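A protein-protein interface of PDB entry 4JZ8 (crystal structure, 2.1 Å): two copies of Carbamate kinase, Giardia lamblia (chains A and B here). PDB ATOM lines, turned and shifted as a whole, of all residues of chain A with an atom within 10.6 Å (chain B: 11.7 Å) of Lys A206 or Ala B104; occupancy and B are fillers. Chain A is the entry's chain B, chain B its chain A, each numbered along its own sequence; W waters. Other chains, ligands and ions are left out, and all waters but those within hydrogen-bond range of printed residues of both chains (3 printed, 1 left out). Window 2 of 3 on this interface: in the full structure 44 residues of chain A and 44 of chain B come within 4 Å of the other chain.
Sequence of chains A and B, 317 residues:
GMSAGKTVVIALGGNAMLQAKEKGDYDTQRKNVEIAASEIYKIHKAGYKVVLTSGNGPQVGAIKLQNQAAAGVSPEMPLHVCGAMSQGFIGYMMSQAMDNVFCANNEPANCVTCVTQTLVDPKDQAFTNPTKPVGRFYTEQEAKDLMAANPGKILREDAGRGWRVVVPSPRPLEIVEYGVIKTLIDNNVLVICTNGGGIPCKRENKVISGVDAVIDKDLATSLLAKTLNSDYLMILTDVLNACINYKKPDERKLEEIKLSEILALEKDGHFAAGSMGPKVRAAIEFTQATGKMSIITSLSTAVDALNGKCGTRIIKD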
ATOM      1  N   GLN A 117     -12.754  25.644  19.823  1.00  0.00           N
ATOM      2  CA  GLN A 117     -13.249  25.429  18.465  1.00  0.00           C
ATOM      3  C   GLN A 117     -13.322  23.937  18.211  1.00  0.00           C
ATOM      4  O   GLN A 117     -12.513  23.149  18.733  1.00  0.00           O
ATOM      5  CB  GLN A 117     -12.329  26.095  17.427  1.00  0.00           C
ATOM      6  CG  GLN A 117     -11.914  27.536  17.757  1.00  0.00           C
ATOM      7  CD  GLN A 117     -10.746  28.036  16.920  1.00  0.00           C
ATOM      8  OE1 GLN A 117     -10.944  28.649  15.861  1.00  0.00           O
ATOM      9  NE2 GLN A 117      -9.500  27.769  17.390  1.00  0.00           N
ATOM     10  N   LEU A 119     -13.637  21.443  14.801  1.00  0.00           N
ATOM     11  CA  LEU A 119     -13.712  21.245  13.357  1.00  0.00           C
ATOM     12  C   LEU A 119     -14.887  20.321  12.997  1.00  0.00           C
ATOM     13  O   LEU A 119     -15.125  19.269  13.654  1.00  0.00           O
ATOM     14  CB  LEU A 119     -12.401  20.661  12.809  1.00  0.00           C
ATOM     15  CG  LEU A 119     -11.109  21.359  13.250  1.00  0.00           C
ATOM     16  CD1 LEU A 119      -9.930  20.909  12.407  1.00  0.00           C
ATOM     17  CD2 LEU A 119     -11.231  22.865  13.159  1.00  0.00           C
ATOM     18  N   VAL A 176      -9.900  21.554  18.522  1.00  0.00           N
ATOM     19  CA  VAL A 176      -8.648  22.196  18.192  1.00  0.00           C
ATOM     20  C   VAL A 176      -7.797  22.401  19.441  1.00  0.00           C
ATOM     21  O   VAL A 176      -6.581  22.245  19.407  1.00  0.00           O
ATOM     22  CB  VAL A 176      -8.884  23.557  17.543  1.00  0.00           C
ATOM     23  CG1 VAL A 176      -7.519  24.270  17.280  1.00  0.00           C
ATOM     24  CG2 VAL A 176      -9.726  23.423  16.259  1.00  0.00           C
ATOM     25  N   CYS A 201     -16.261  25.014  13.285  1.00  0.00           N
ATOM     26  CA  CYS A 201     -15.302  25.531  12.314  1.00  0.00           C
ATOM     27  C   CYS A 201     -14.998  24.511  11.216  1.00  0.00           C
ATOM     28  O   CYS A 201     -15.134  23.307  11.415  1.00  0.00           O
ATOM     29  CB  CYS A 201     -13.978  25.860  13.025  1.00  0.00           C
ATOM     30  SG  CYS A 201     -13.980  27.276  14.183  1.00  0.00           S
ATOM     31  N   LYS A 202     -14.539  24.982  10.066  1.00  0.00           N
ATOM     32  CA  LYS A 202     -13.977  24.073   9.069  1.00  0.00           C
ATOM     33  C   LYS A 202     -12.479  24.345   8.965  1.00  0.00           C
ATOM     34  O   LYS A 202     -12.007  25.431   9.320  1.00  0.00           O
ATOM     35  CB  LYS A 202     -14.666  24.220   7.706  1.00  0.00           C
ATOM     36  CG  LYS A 202     -14.355  25.531   6.987  1.00  0.00           C
ATOM     37  CD  LYS A 202     -15.270  25.742   5.767  1.00  0.00           C
ATOM     38  CE  LYS A 202     -15.019  27.124   5.124  1.00  0.00           C
ATOM     39  NZ  LYS A 202     -15.652  27.264   3.758  1.00  0.00           N
ATOM     40  N   ARG A 203     -11.721  23.347   8.535  1.00  0.00           N
ATOM     41  CA  ARG A 203     -10.327  23.588   8.213  1.00  0.00           C
ATOM     42  C   ARG A 203     -10.028  23.314   6.732  1.00  0.00           C
ATOM     43  O   ARG A 203      -9.981  22.150   6.303  1.00  0.00           O
ATOM     44  CB  ARG A 203      -9.390  22.781   9.110  1.00  0.00           C
ATOM     45  CG  ARG A 203      -7.925  23.026   8.748  1.00  0.00           C
ATOM     46  CD  ARG A 203      -7.033  22.707   9.909  1.00  0.00           C
ATOM     47  NE  ARG A 203      -7.101  21.292  10.269  1.00  0.00           N
ATOM     48  CZ  ARG A 203      -6.691  20.819  11.436  1.00  0.00           C
ATOM     49  NH1 ARG A 203      -6.211  21.656  12.346  1.00  0.00           N
ATOM     50  NH2 ARG A 203      -6.766  19.521  11.695  1.00  0.00           N
ATOM     51  N   GLU A 204      -9.843  24.392   5.968  1.00  0.00           N
ATOM     52  CA  GLU A 204      -9.482  24.320   4.552  1.00  0.00           C
ATOM     53  C   GLU A 204      -8.138  25.008   4.273  1.00  0.00           C
ATOM     54  O   GLU A 204      -7.873  26.102   4.787  1.00  0.00           O
ATOM     55  CB  GLU A 204     -10.553  24.992   3.685  1.00  0.00           C
ATOM     56  CG  GLU A 204     -11.818  24.213   3.521  1.00  0.00           C
ATOM     57  CD  GLU A 204     -12.916  25.050   2.897  1.00  0.00           C
ATOM     58  OE1 GLU A 204     -12.796  26.297   2.970  1.00  0.00           O
ATOM     59  OE2 GLU A 204     -13.884  24.472   2.337  1.00  0.00           O
ATOM     60  N   ASN A 205      -7.307  24.381   3.437  1.00  0.00           N
ATOM     61  CA  ASN A 205      -6.041  24.981   3.043  1.00  0.00           C
ATOM     62  C   ASN A 205      -5.285  25.439   4.278  1.00  0.00           C
ATOM     63  O   ASN A 205      -4.669  26.501   4.273  1.00  0.00           O
ATOM     64  CB  ASN A 205      -6.287  26.203   2.152  1.00  0.00           C
ATOM     65  CG  ASN A 205      -6.666  25.828   0.740  1.00  0.00           C
ATOM     66  OD1 ASN A 205      -7.848  25.623   0.431  1.00  0.00           O
ATOM     67  ND2 ASN A 205      -5.663  25.748  -0.137  1.00  0.00           N
ATOM     68  N   LYS A 206      -5.378  24.664   5.352  1.00  0.00           N
ATOM     69  CA  LYS A 206      -4.717  25.027   6.606  1.00  0.00           C
ATOM     70  C   LYS A 206      -5.316  26.297   7.230  1.00  0.00           C
ATOM     71  O   LYS A 206      -4.710  26.933   8.095  1.00  0.00           O
ATOM     72  CB  LYS A 206      -3.209  25.181   6.382  1.00  0.00           C
ATOM     73  CG  LYS A 206      -2.462  23.855   6.347  1.00  0.00           C
ATOM     74  CD  LYS A 206      -1.216  23.937   5.465  1.00  0.00           C
ATOM     75  CE  LYS A 206      -0.954  25.361   5.007  1.00  0.00           C
ATOM     76  NZ  LYS A 206       0.502  25.705   5.050  1.00  0.00           N
ATOM     77  N   VAL A 207      -6.509  26.662   6.787  1.00  0.00           N
ATOM     78  CA  VAL A 207      -7.166  27.844   7.318  1.00  0.00           C
ATOM     79  C   VAL A 207      -8.412  27.407   8.055  1.00  0.00           C
ATOM     80  O   VAL A 207      -9.340  26.906   7.446  1.00  0.00           O
ATOM     81  CB  VAL A 207      -7.532  28.835   6.199  1.00  0.00           C
ATOM     82  CG1 VAL A 207      -8.359  30.027   6.747  1.00  0.00           C
ATOM     83  CG2 VAL A 207      -6.250  29.322   5.499  1.00  0.00           C
ATOM     84  N   ILE A 208      -8.381  27.554   9.379  1.00  0.00           N
ATOM     85  CA  ILE A 208      -9.549  27.383  10.223  1.00  0.00           C
ATOM     86  C   ILE A 208     -10.413  28.636  10.070  1.00  0.00           C
ATOM     87  O   ILE A 208      -9.960  29.751  10.362  1.00  0.00           O
ATOM     88  CB  ILE A 208      -9.160  27.264  11.723  1.00  0.00           C
ATOM     89  CG1 ILE A 208      -8.335  25.987  11.990  1.00  0.00           C
ATOM     90  CG2 ILE A 208     -10.433  27.311  12.622  1.00  0.00           C
ATOM     91  CD1 ILE A 208      -7.669  25.962  13.382  1.00  0.00           C
ATOM     92  N   SER A 209     -11.647  28.461   9.608  1.00  0.00           N
ATOM     93  CA  SER A 209     -12.616  29.561   9.615  1.00  0.00           C
ATOM     94  C   SER A 209     -13.925  29.038  10.206  1.00  0.00           C
ATOM     95  O   SER A 209     -14.150  27.826  10.211  1.00  0.00           O
ATOM     96  CB  SER A 209     -12.840  30.104   8.205  1.00  0.00           C
ATOM     97  OG  SER A 209     -13.443  29.134   7.362  1.00  0.00           O
ATOM     98  N   GLU B  34      -6.304  39.144  12.002  1.00  0.00           N
ATOM     99  CA  GLU B  34      -5.320  38.431  11.184  1.00  0.00           C
ATOM    100  C   GLU B  34      -4.036  39.235  11.036  1.00  0.00           C
ATOM    101  O   GLU B  34      -2.934  38.706  11.159  1.00  0.00           O
ATOM    102  CB  GLU B  34      -5.912  38.051   9.821  1.00  0.00           C
ATOM    103  CG  GLU B  34      -6.639  36.716   9.888  1.00  0.00           C
ATOM    104  CD  GLU B  34      -7.788  36.582   8.900  1.00  0.00           C
ATOM    105  OE1 GLU B  34      -7.881  37.422   7.979  1.00  0.00           O
ATOM    106  OE2 GLU B  34      -8.604  35.641   9.066  1.00  0.00           O
ATOM    107  N   ALA B  37      -2.225  39.201  14.360  1.00  0.00           N
ATOM    108  CA  ALA B  37      -1.648  37.883  14.561  1.00  0.00           C
ATOM    109  C   ALA B  37      -0.279  37.704  13.851  1.00  0.00           C
ATOM    110  O   ALA B  37       0.673  37.157  14.450  1.00  0.00           O
ATOM    111  CB  ALA B  37      -2.643  36.802  14.161  1.00  0.00           C
ATOM    112  N   SER B  38      -0.159  38.190  12.613  1.00  0.00           N
ATOM    113  CA  SER B  38       1.116  38.115  11.878  1.00  0.00           C
ATOM    114  C   SER B  38       2.224  38.762  12.674  1.00  0.00           C
ATOM    115  O   SER B  38       3.328  38.213  12.782  1.00  0.00           O
ATOM    116  CB  SER B  38       1.047  38.774  10.478  1.00  0.00           C
ATOM    117  OG  SER B  38       0.044  38.181   9.657  1.00  0.00           O
ATOM    118  N   GLU B  39       1.951  39.939  13.222  1.00  0.00           N
ATOM    119  CA  GLU B  39       2.998  40.627  13.972  1.00  0.00           C
ATOM    120  C   GLU B  39       3.359  39.832  15.197  1.00  0.00           C
ATOM    121  O   GLU B  39       4.528  39.652  15.501  1.00  0.00           O
ATOM    122  CB  GLU B  39       2.605  42.061  14.333  1.00  0.00           C
ATOM    123  CG  GLU B  39       2.920  43.011  13.227  1.00  0.00           C
ATOM    124  CD  GLU B  39       4.355  42.825  12.750  1.00  0.00           C
ATOM    125  OE1 GLU B  39       5.294  43.177  13.505  1.00  0.00           O
ATOM    126  OE2 GLU B  39       4.536  42.295  11.626  1.00  0.00           O
ATOM    127  N   TYR B  41       3.053  36.645  15.671  1.00  0.00           N
ATOM    128  CA  TYR B  41       3.761  35.416  15.346  1.00  0.00           C
ATOM    129  C   TYR B  41       5.257  35.614  15.377  1.00  0.00           C
ATOM    130  O   TYR B  41       6.006  34.708  15.774  1.00  0.00           O
ATOM    131  CB  TYR B  41       3.390  34.837  13.989  1.00  0.00           C
ATOM    132  CG  TYR B  41       3.984  33.460  13.846  1.00  0.00           C
ATOM    133  CD1 TYR B  41       3.416  32.373  14.508  1.00  0.00           C
ATOM    134  CD2 TYR B  41       5.133  33.244  13.090  1.00  0.00           C
ATOM    135  CE1 TYR B  41       3.951  31.117  14.399  1.00  0.00           C
ATOM    136  CE2 TYR B  41       5.685  31.966  12.975  1.00  0.00           C
ATOM    137  CZ  TYR B  41       5.086  30.917  13.635  1.00  0.00           C
ATOM    138  OH  TYR B  41       5.593  29.655  13.540  1.00  0.00           O
ATOM    139  N   LYS B  42       5.685  36.784  14.937  1.00  0.00           N
ATOM    140  CA  LYS B  42       7.111  37.066  14.848  1.00  0.00           C
ATOM    141  C   LYS B  42       7.753  37.097  16.234  1.00  0.00           C
ATOM    142  O   LYS B  42       8.949  36.824  16.363  1.00  0.00           O
ATOM    143  CB  LYS B  42       7.353  38.405  14.137  1.00  0.00           C
ATOM    144  CG  LYS B  42       6.828  38.499  12.710  1.00  0.00           C
ATOM    145  CD  LYS B  42       6.618  39.975  12.373  1.00  0.00           C
ATOM    146  CE  LYS B  42       6.573  40.212  10.879  1.00  0.00           C
ATOM    147  NZ  LYS B  42       6.413  41.689  10.580  1.00  0.00           N
ATOM    148  N   HIS B  44       6.632  35.242  18.883  1.00  0.00           N
ATOM    149  CA  HIS B  44       6.700  33.821  19.201  1.00  0.00           C
ATOM    150  C   HIS B  44       7.843  33.164  18.425  1.00  0.00           C
ATOM    151  O   HIS B  44       8.445  32.181  18.881  1.00  0.00           O
ATOM    152  CB  HIS B  44       5.410  33.129  18.814  1.00  0.00           C
ATOM    153  CG  HIS B  44       5.434  31.641  19.012  1.00  0.00           C
ATOM    154  ND1 HIS B  44       5.378  31.052  20.261  1.00  0.00           N
ATOM    155  CD2 HIS B  44       5.514  30.628  18.122  1.00  0.00           C
ATOM    156  CE1 HIS B  44       5.401  29.737  20.126  1.00  0.00           C
ATOM    157  NE2 HIS B  44       5.486  29.452  18.836  1.00  0.00           N
ATOM    158  N   LYS B  45       8.130  33.678  17.231  1.00  0.00           N
ATOM    159  CA  LYS B  45       9.063  32.950  16.417  1.00  0.00           C
ATOM    160  C   LYS B  45      10.488  33.344  16.846  1.00  0.00           C
ATOM    161  O   LYS B  45      11.374  32.504  16.860  1.00  0.00           O
ATOM    162  CB  LYS B  45       8.793  33.098  14.927  1.00  0.00           C
ATOM    163  CG  LYS B  45       9.383  31.958  14.090  1.00  0.00           C
ATOM    164  CD  LYS B  45       9.436  32.314  12.610  1.00  0.00           C
ATOM    165  CE  LYS B  45       9.986  31.151  11.774  1.00  0.00           C
ATOM    166  NZ  LYS B  45       8.903  30.253  11.254  1.00  0.00           N
ATOM    167  N   SER B  95      -7.538  33.612  18.896  1.00  0.00           N
ATOM    168  CA  SER B  95      -7.025  32.222  18.947  1.00  0.00           C
ATOM    169  C   SER B  95      -7.000  31.560  17.576  1.00  0.00           C
ATOM    170  O   SER B  95      -6.011  30.892  17.194  1.00  0.00           O
ATOM    171  CB  SER B  95      -7.903  31.369  19.857  1.00  0.00           C
ATOM    172  OG  SER B  95      -7.751  31.757  21.204  1.00  0.00           O
ATOM    173  N   GLN B  96      -8.100  31.737  16.854  1.00  0.00           N
ATOM    174  CA  GLN B  96      -8.247  31.248  15.479  1.00  0.00           C
ATOM    175  C   GLN B  96      -7.186  31.860  14.590  1.00  0.00           C
ATOM    176  O   GLN B  96      -6.514  31.162  13.813  1.00  0.00           O
ATOM    177  CB  GLN B  96      -9.631  31.646  14.923  1.00  0.00           C
ATOM    178  CG  GLN B  96      -9.791  31.215  13.490  1.00  0.00           C
ATOM    179  CD  GLN B  96     -11.224  31.319  13.008  1.00  0.00           C
ATOM    180  OE1 GLN B  96     -11.585  32.274  12.334  1.00  0.00           O
ATOM    181  NE2 GLN B  96     -12.043  30.323  13.338  1.00  0.00           N
ATOM    182  N   ALA B  97      -7.044  33.179  14.711  1.00  0.00           N
ATOM    183  CA  ALA B  97      -6.039  33.905  13.950  1.00  0.00           C
ATOM    184  C   ALA B  97      -4.677  33.352  14.307  1.00  0.00           C
ATOM    185  O   ALA B  97      -3.938  32.956  13.406  1.00  0.00           O
ATOM    186  CB  ALA B  97      -6.105  35.410  14.226  1.00  0.00           C
ATOM    187  N   MET B  98      -4.339  33.304  15.608  1.00  0.00           N
ATOM    188  CA  MET B  98      -3.030  32.740  16.032  1.00  0.00           C
ATOM    189  C   MET B  98      -2.889  31.317  15.519  1.00  0.00           C
ATOM    190  O   MET B  98      -1.857  30.963  14.954  1.00  0.00           O
ATOM    191  CB  MET B  98      -2.748  32.804  17.557  1.00  0.00           C
ATOM    192  CG  MET B  98      -2.573  34.242  18.142  1.00  0.00           C
ATOM    193  SD  MET B  98      -1.404  35.343  17.259  1.00  0.00           S
ATOM    194  CE  MET B  98       0.094  34.296  17.112  1.00  0.00           C
ATOM    195  N   ASP B  99      -3.918  30.493  15.691  1.00  0.00           N
ATOM    196  CA  ASP B  99      -3.865  29.146  15.125  1.00  0.00           C
ATOM    197  C   ASP B  99      -3.463  29.197  13.631  1.00  0.00           C
ATOM    198  O   ASP B  99      -2.487  28.581  13.225  1.00  0.00           O
ATOM    199  CB  ASP B  99      -5.192  28.414  15.314  1.00  0.00           C
ATOM    200  CG  ASP B  99      -5.450  28.037  16.764  1.00  0.00           C
ATOM    201  OD1 ASP B  99      -6.551  27.535  17.052  1.00  0.00           O
ATOM    202  OD2 ASP B  99      -4.543  28.209  17.611  1.00  0.00           O
ATOM    203  N   ASN B 100      -4.187  29.971  12.830  1.00  0.00           N
ATOM    204  CA  ASN B 100      -3.900  30.031  11.400  1.00  0.00           C
ATOM    205  C   ASN B 100      -2.460  30.399  11.026  1.00  0.00           C
ATOM    206  O   ASN B 100      -1.859  29.773  10.136  1.00  0.00           O
ATOM    207  CB  ASN B 100      -4.903  30.944  10.697  1.00  0.00           C
ATOM    208  CG  ASN B 100      -6.308  30.367  10.727  1.00  0.00           C
ATOM    209  OD1 ASN B 100      -6.474  29.176  10.956  1.00  0.00           O
ATOM    210  ND2 ASN B 100      -7.314  31.197  10.490  1.00  0.00           N
ATOM    211  N   VAL B 101      -1.901  31.410  11.689  1.00  0.00           N
ATOM    212  CA  VAL B 101      -0.556  31.840  11.352  1.00  0.00           C
ATOM    213  C   VAL B 101       0.476  30.783  11.809  1.00  0.00           C
ATOM    214  O   VAL B 101       1.525  30.606  11.179  1.00  0.00           O
ATOM    215  CB  VAL B 101      -0.275  33.242  11.920  1.00  0.00           C
ATOM    216  CG1 VAL B 101      -0.051  33.172  13.421  1.00  0.00           C
ATOM    217  CG2 VAL B 101       0.895  33.898  11.212  1.00  0.00           C
ATOM    218  N   PHE B 102       0.155  30.045  12.872  1.00  0.00           N
ATOM    219  CA  PHE B 102       1.001  28.931  13.326  1.00  0.00           C
ATOM    220  C   PHE B 102       1.027  27.835  12.263  1.00  0.00           C
ATOM    221  O   PHE B 102       2.080  27.263  11.950  1.00  0.00           O
ATOM    222  CB  PHE B 102       0.462  28.327  14.628  1.00  0.00           C
ATOM    223  CG  PHE B 102       1.051  28.922  15.877  1.00  0.00           C
ATOM    224  CD1 PHE B 102       0.810  30.244  16.208  1.00  0.00           C
ATOM    225  CD2 PHE B 102       1.824  28.153  16.735  1.00  0.00           C
ATOM    226  CE1 PHE B 102       1.348  30.806  17.366  1.00  0.00           C
ATOM    227  CE2 PHE B 102       2.354  28.702  17.900  1.00  0.00           C
ATOM    228  CZ  PHE B 102       2.115  30.044  18.213  1.00  0.00           C
ATOM    229  N   CYS B 103      -0.152  27.532  11.729  1.00  0.00           N
ATOM    230  CA  CYS B 103      -0.304  26.468  10.733  1.00  0.00           C
ATOM    231  C   CYS B 103       0.362  26.882   9.426  1.00  0.00           C
ATOM    232  O   CYS B 103       1.111  26.118   8.825  1.00  0.00           O
ATOM    233  CB  CYS B 103      -1.791  26.148  10.499  1.00  0.00           C
ATOM    234  SG  CYS B 103      -2.176  24.599   9.502  1.00  0.00           S
ATOM    235  N   ALA B 104       0.082  28.099   8.995  1.00  0.00           N
ATOM    236  CA  ALA B 104       0.639  28.597   7.763  1.00  0.00           C
ATOM    237  C   ALA B 104       2.147  28.383   7.788  1.00  0.00           C
ATOM    238  O   ALA B 104       2.737  28.114   6.752  1.00  0.00           O
ATOM    239  CB  ALA B 104       0.296  30.073   7.586  1.00  0.00           C
ATOM    240  N   ASN B 105       2.748  28.490   8.976  1.00  0.00           N
ATOM    241  CA  ASN B 105       4.195  28.310   9.170  1.00  0.00           C
ATOM    242  C   ASN B 105       4.577  26.900   9.606  1.00  0.00           C
ATOM    243  O   ASN B 105       5.577  26.700  10.317  1.00  0.00           O
ATOM    244  CB  ASN B 105       4.729  29.302  10.207  1.00  0.00           C
ATOM    245  CG  ASN B 105       4.734  30.730   9.702  1.00  0.00           C
ATOM    246  OD1 ASN B 105       5.758  31.223   9.230  1.00  0.00           O
ATOM    247  ND2 ASN B 105       3.588  31.410   9.808  1.00  0.00           N
ATOM    248  N   ASN B 106       3.766  25.928   9.197  1.00  0.00           N
ATOM    249  CA  ASN B 106       3.933  24.538   9.611  1.00  0.00           C
ATOM    250  C   ASN B 106       4.348  24.401  11.082  1.00  0.00           C
ATOM    251  O   ASN B 106       5.172  23.553  11.447  1.00  0.00           O
ATOM    252  CB  ASN B 106       4.920  23.812   8.686  1.00  0.00           C
ATOM    253  CG  ASN B 106       4.545  23.934   7.210  1.00  0.00           C
ATOM    254  OD1 ASN B 106       3.500  23.437   6.769  1.00  0.00           O
ATOM    255  ND2 ASN B 106       5.405  24.594   6.438  1.00  0.00           N
ATOM    256  N   GLU B 107       3.783  25.251  11.926  1.00  0.00           N
ATOM    257  CA  GLU B 107       3.929  25.098  13.369  1.00  0.00           C
ATOM    258  C   GLU B 107       2.566  24.722  13.971  1.00  0.00           C
ATOM    259  O   GLU B 107       1.552  25.407  13.735  1.00  0.00           O
ATOM    260  CB  GLU B 107       4.491  26.374  14.003  1.00  0.00           C
ATOM    261  CG  GLU B 107       4.660  26.279  15.489  1.00  0.00           C
ATOM    262  CD  GLU B 107       5.465  27.422  16.086  1.00  0.00           C
ATOM    263  OE1 GLU B 107       5.563  27.452  17.331  1.00  0.00           O
ATOM    264  OE2 GLU B 107       6.017  28.265  15.334  1.00  0.00           O
ATOM    265  N   PRO B 108       2.531  23.619  14.733  1.00  0.00           N
ATOM    266  CA  PRO B 108       1.267  23.173  15.335  1.00  0.00           C
ATOM    267  C   PRO B 108       0.700  24.192  16.317  1.00  0.00           C
ATOM    268  O   PRO B 108       1.457  24.839  17.065  1.00  0.00           O
ATOM    269  CB  PRO B 108       1.641  21.877  16.077  1.00  0.00           C
ATOM    270  CG  PRO B 108       3.160  21.900  16.202  1.00  0.00           C
ATOM    271  CD  PRO B 108       3.660  22.715  15.036  1.00  0.00           C
ATOM    272  N   ALA B 109      -0.626  24.319  16.294  1.00  0.00           N
ATOM    273  CA  ALA B 109      -1.360  25.219  17.169  1.00  0.00           C
ATOM    274  C   ALA B 109      -1.061  24.917  18.633  1.00  0.00           C
ATOM    275  O   ALA B 109      -1.114  23.765  19.059  1.00  0.00           O
ATOM    276  CB  ALA B 109      -2.864  25.110  16.899  1.00  0.00           C
ATOM    277  N   ASN B 110      -0.756  25.962  19.402  1.00  0.00           N
ATOM    278  CA  ASN B 110      -0.503  25.823  20.826  1.00  0.00           C
ATOM    279  C   ASN B 110      -0.964  27.085  21.538  1.00  0.00           C
ATOM    280  O   ASN B 110      -0.172  27.796  22.154  1.00  0.00           O
ATOM    281  CB  ASN B 110       0.983  25.575  21.078  1.00  0.00           C
ATOM    282  CG  ASN B 110       1.240  25.098  22.470  1.00  0.00           C
ATOM    283  OD1 ASN B 110       0.373  24.435  23.069  1.00  0.00           O
ATOM    284  ND2 ASN B 110       2.423  25.425  23.019  1.00  0.00           N
HETATM  285  O   HOH W   1     -10.737  32.325   9.359  1.00  0.00           O
HETATM  286  O   HOH W   2      -3.103  29.308   8.030  1.00  0.00           O
HETATM  287  O   HOH W   3       2.662  27.381   4.085  1.00  0.00           O
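The side-chain amide nitrogen (ND2) of Asn B100 lies close to the backbone carbonyl oxygen (O) of Gln B96 (3.4 Å).
The backbone carbonyl oxygen (O) of Gln A117 lies within hydrogen-bond range of the backbone NH (N) of Val A176 (3.1 Å).
The side-chain amide oxygen (OE1) of Gln A117 lies within hydrogen-bond range of the side-chain sulfur (SG) of Cys A201.
N of Lys A202 lies within hydrogen-bond range of O of Ser A209 (2.9 Å).
Water W2 bridges the backbone carbonyl oxygen of Asn B100 (2.5 Å) and the backbone carbonyl oxygen of Lys A206 (2.9 Å).
Water W3 lies within hydrogen-bond range of O of Ala B104 (2.8 Å) and NZ of Lys A206 (2.9 Å).
Water W1 bridges O of Ile A208 (2.9 Å) and OE1 of Gln B96 (3.1 Å).
No position is printed for both chains.
The side-chain amide nitrogen (NE2) of Gln B96 lies within hydrogen-bond range of the side-chain amide oxygen (OE1) of Gln A117, at 3.2 Å.
SG of Cys A201 is in hydrogen-bond range of NE2 of Gln B96, 3.7 Å away.
The side-chain carboxylate (OD1) of Asp B99 is in hydrogen-bond range of the side-chain amide nitrogen (NE2) of Gln A117, 3.0 Å away.
The side-chain amide oxygen (OD1) of Asn B100 sits at hydrogen-bond distance from the backbone NH (N) of Ile A208 (3.0 Å).
O of Lys A206 lies close to SG of Cys B103, at 3.7 Å.
Among the printed residues, merely in contact across the chains: Val A176 with Asp B99 (3.4 Å), Lys A206 with Ala B104 (3.7 Å), Val A207 with Asn B100 (3.9 Å), Ile A208 with Gln B96 (3.3 Å), Ile A208 with Asp B99 (3.99 Å) and Ser A209 with Gln B96 (3.8 Å).
Hydrophobic or aromatic side chains of chain A that line the printed part of chain B: Val A176 and Ile A208.
Of the 24 printed residues of chain B, 5 touch a printed residue of chain A.
Among the printed residues, 11 pairs touch across the chains.
Of chain B, only Cys B103 and Ala B104 come within 4 Å of Lys A206.
Ala B104 touches just one residue of chain A: Lys A206 (3.7 Å).
No residue of chain B comes within 4 Å of Asn A205.
Asn B100 touches two residues of chain A.
Of the printed residues of chain A, Cys B103 touches Lys A206.
No residue of chain A comes within 4 Å of Asn B105.
Of the printed residues of chain B, Ser A209 touches Gln B96 (3.8 Å).
Printed residues of chain B within 4 Å of Gln A117: Gln B96 and Asp B99.
Of the printed residues of chain B, Ile A208 touches Gln B96, Asp B99 and Asn B100.
Of the printed residues of chain B, Val A176 touches Asp B99 (3.4 Å).
Val B101 touches none of the printed residues of chain A.
Pro B108 touches none of the printed residues of chain A.
The nearest residue of chain B that does not touch Lys A206 is Asn B100 (4.04 Å).
The nearest printed residue of chain A that does not touch Asp B99 is Lys A206 (5.8 Å).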
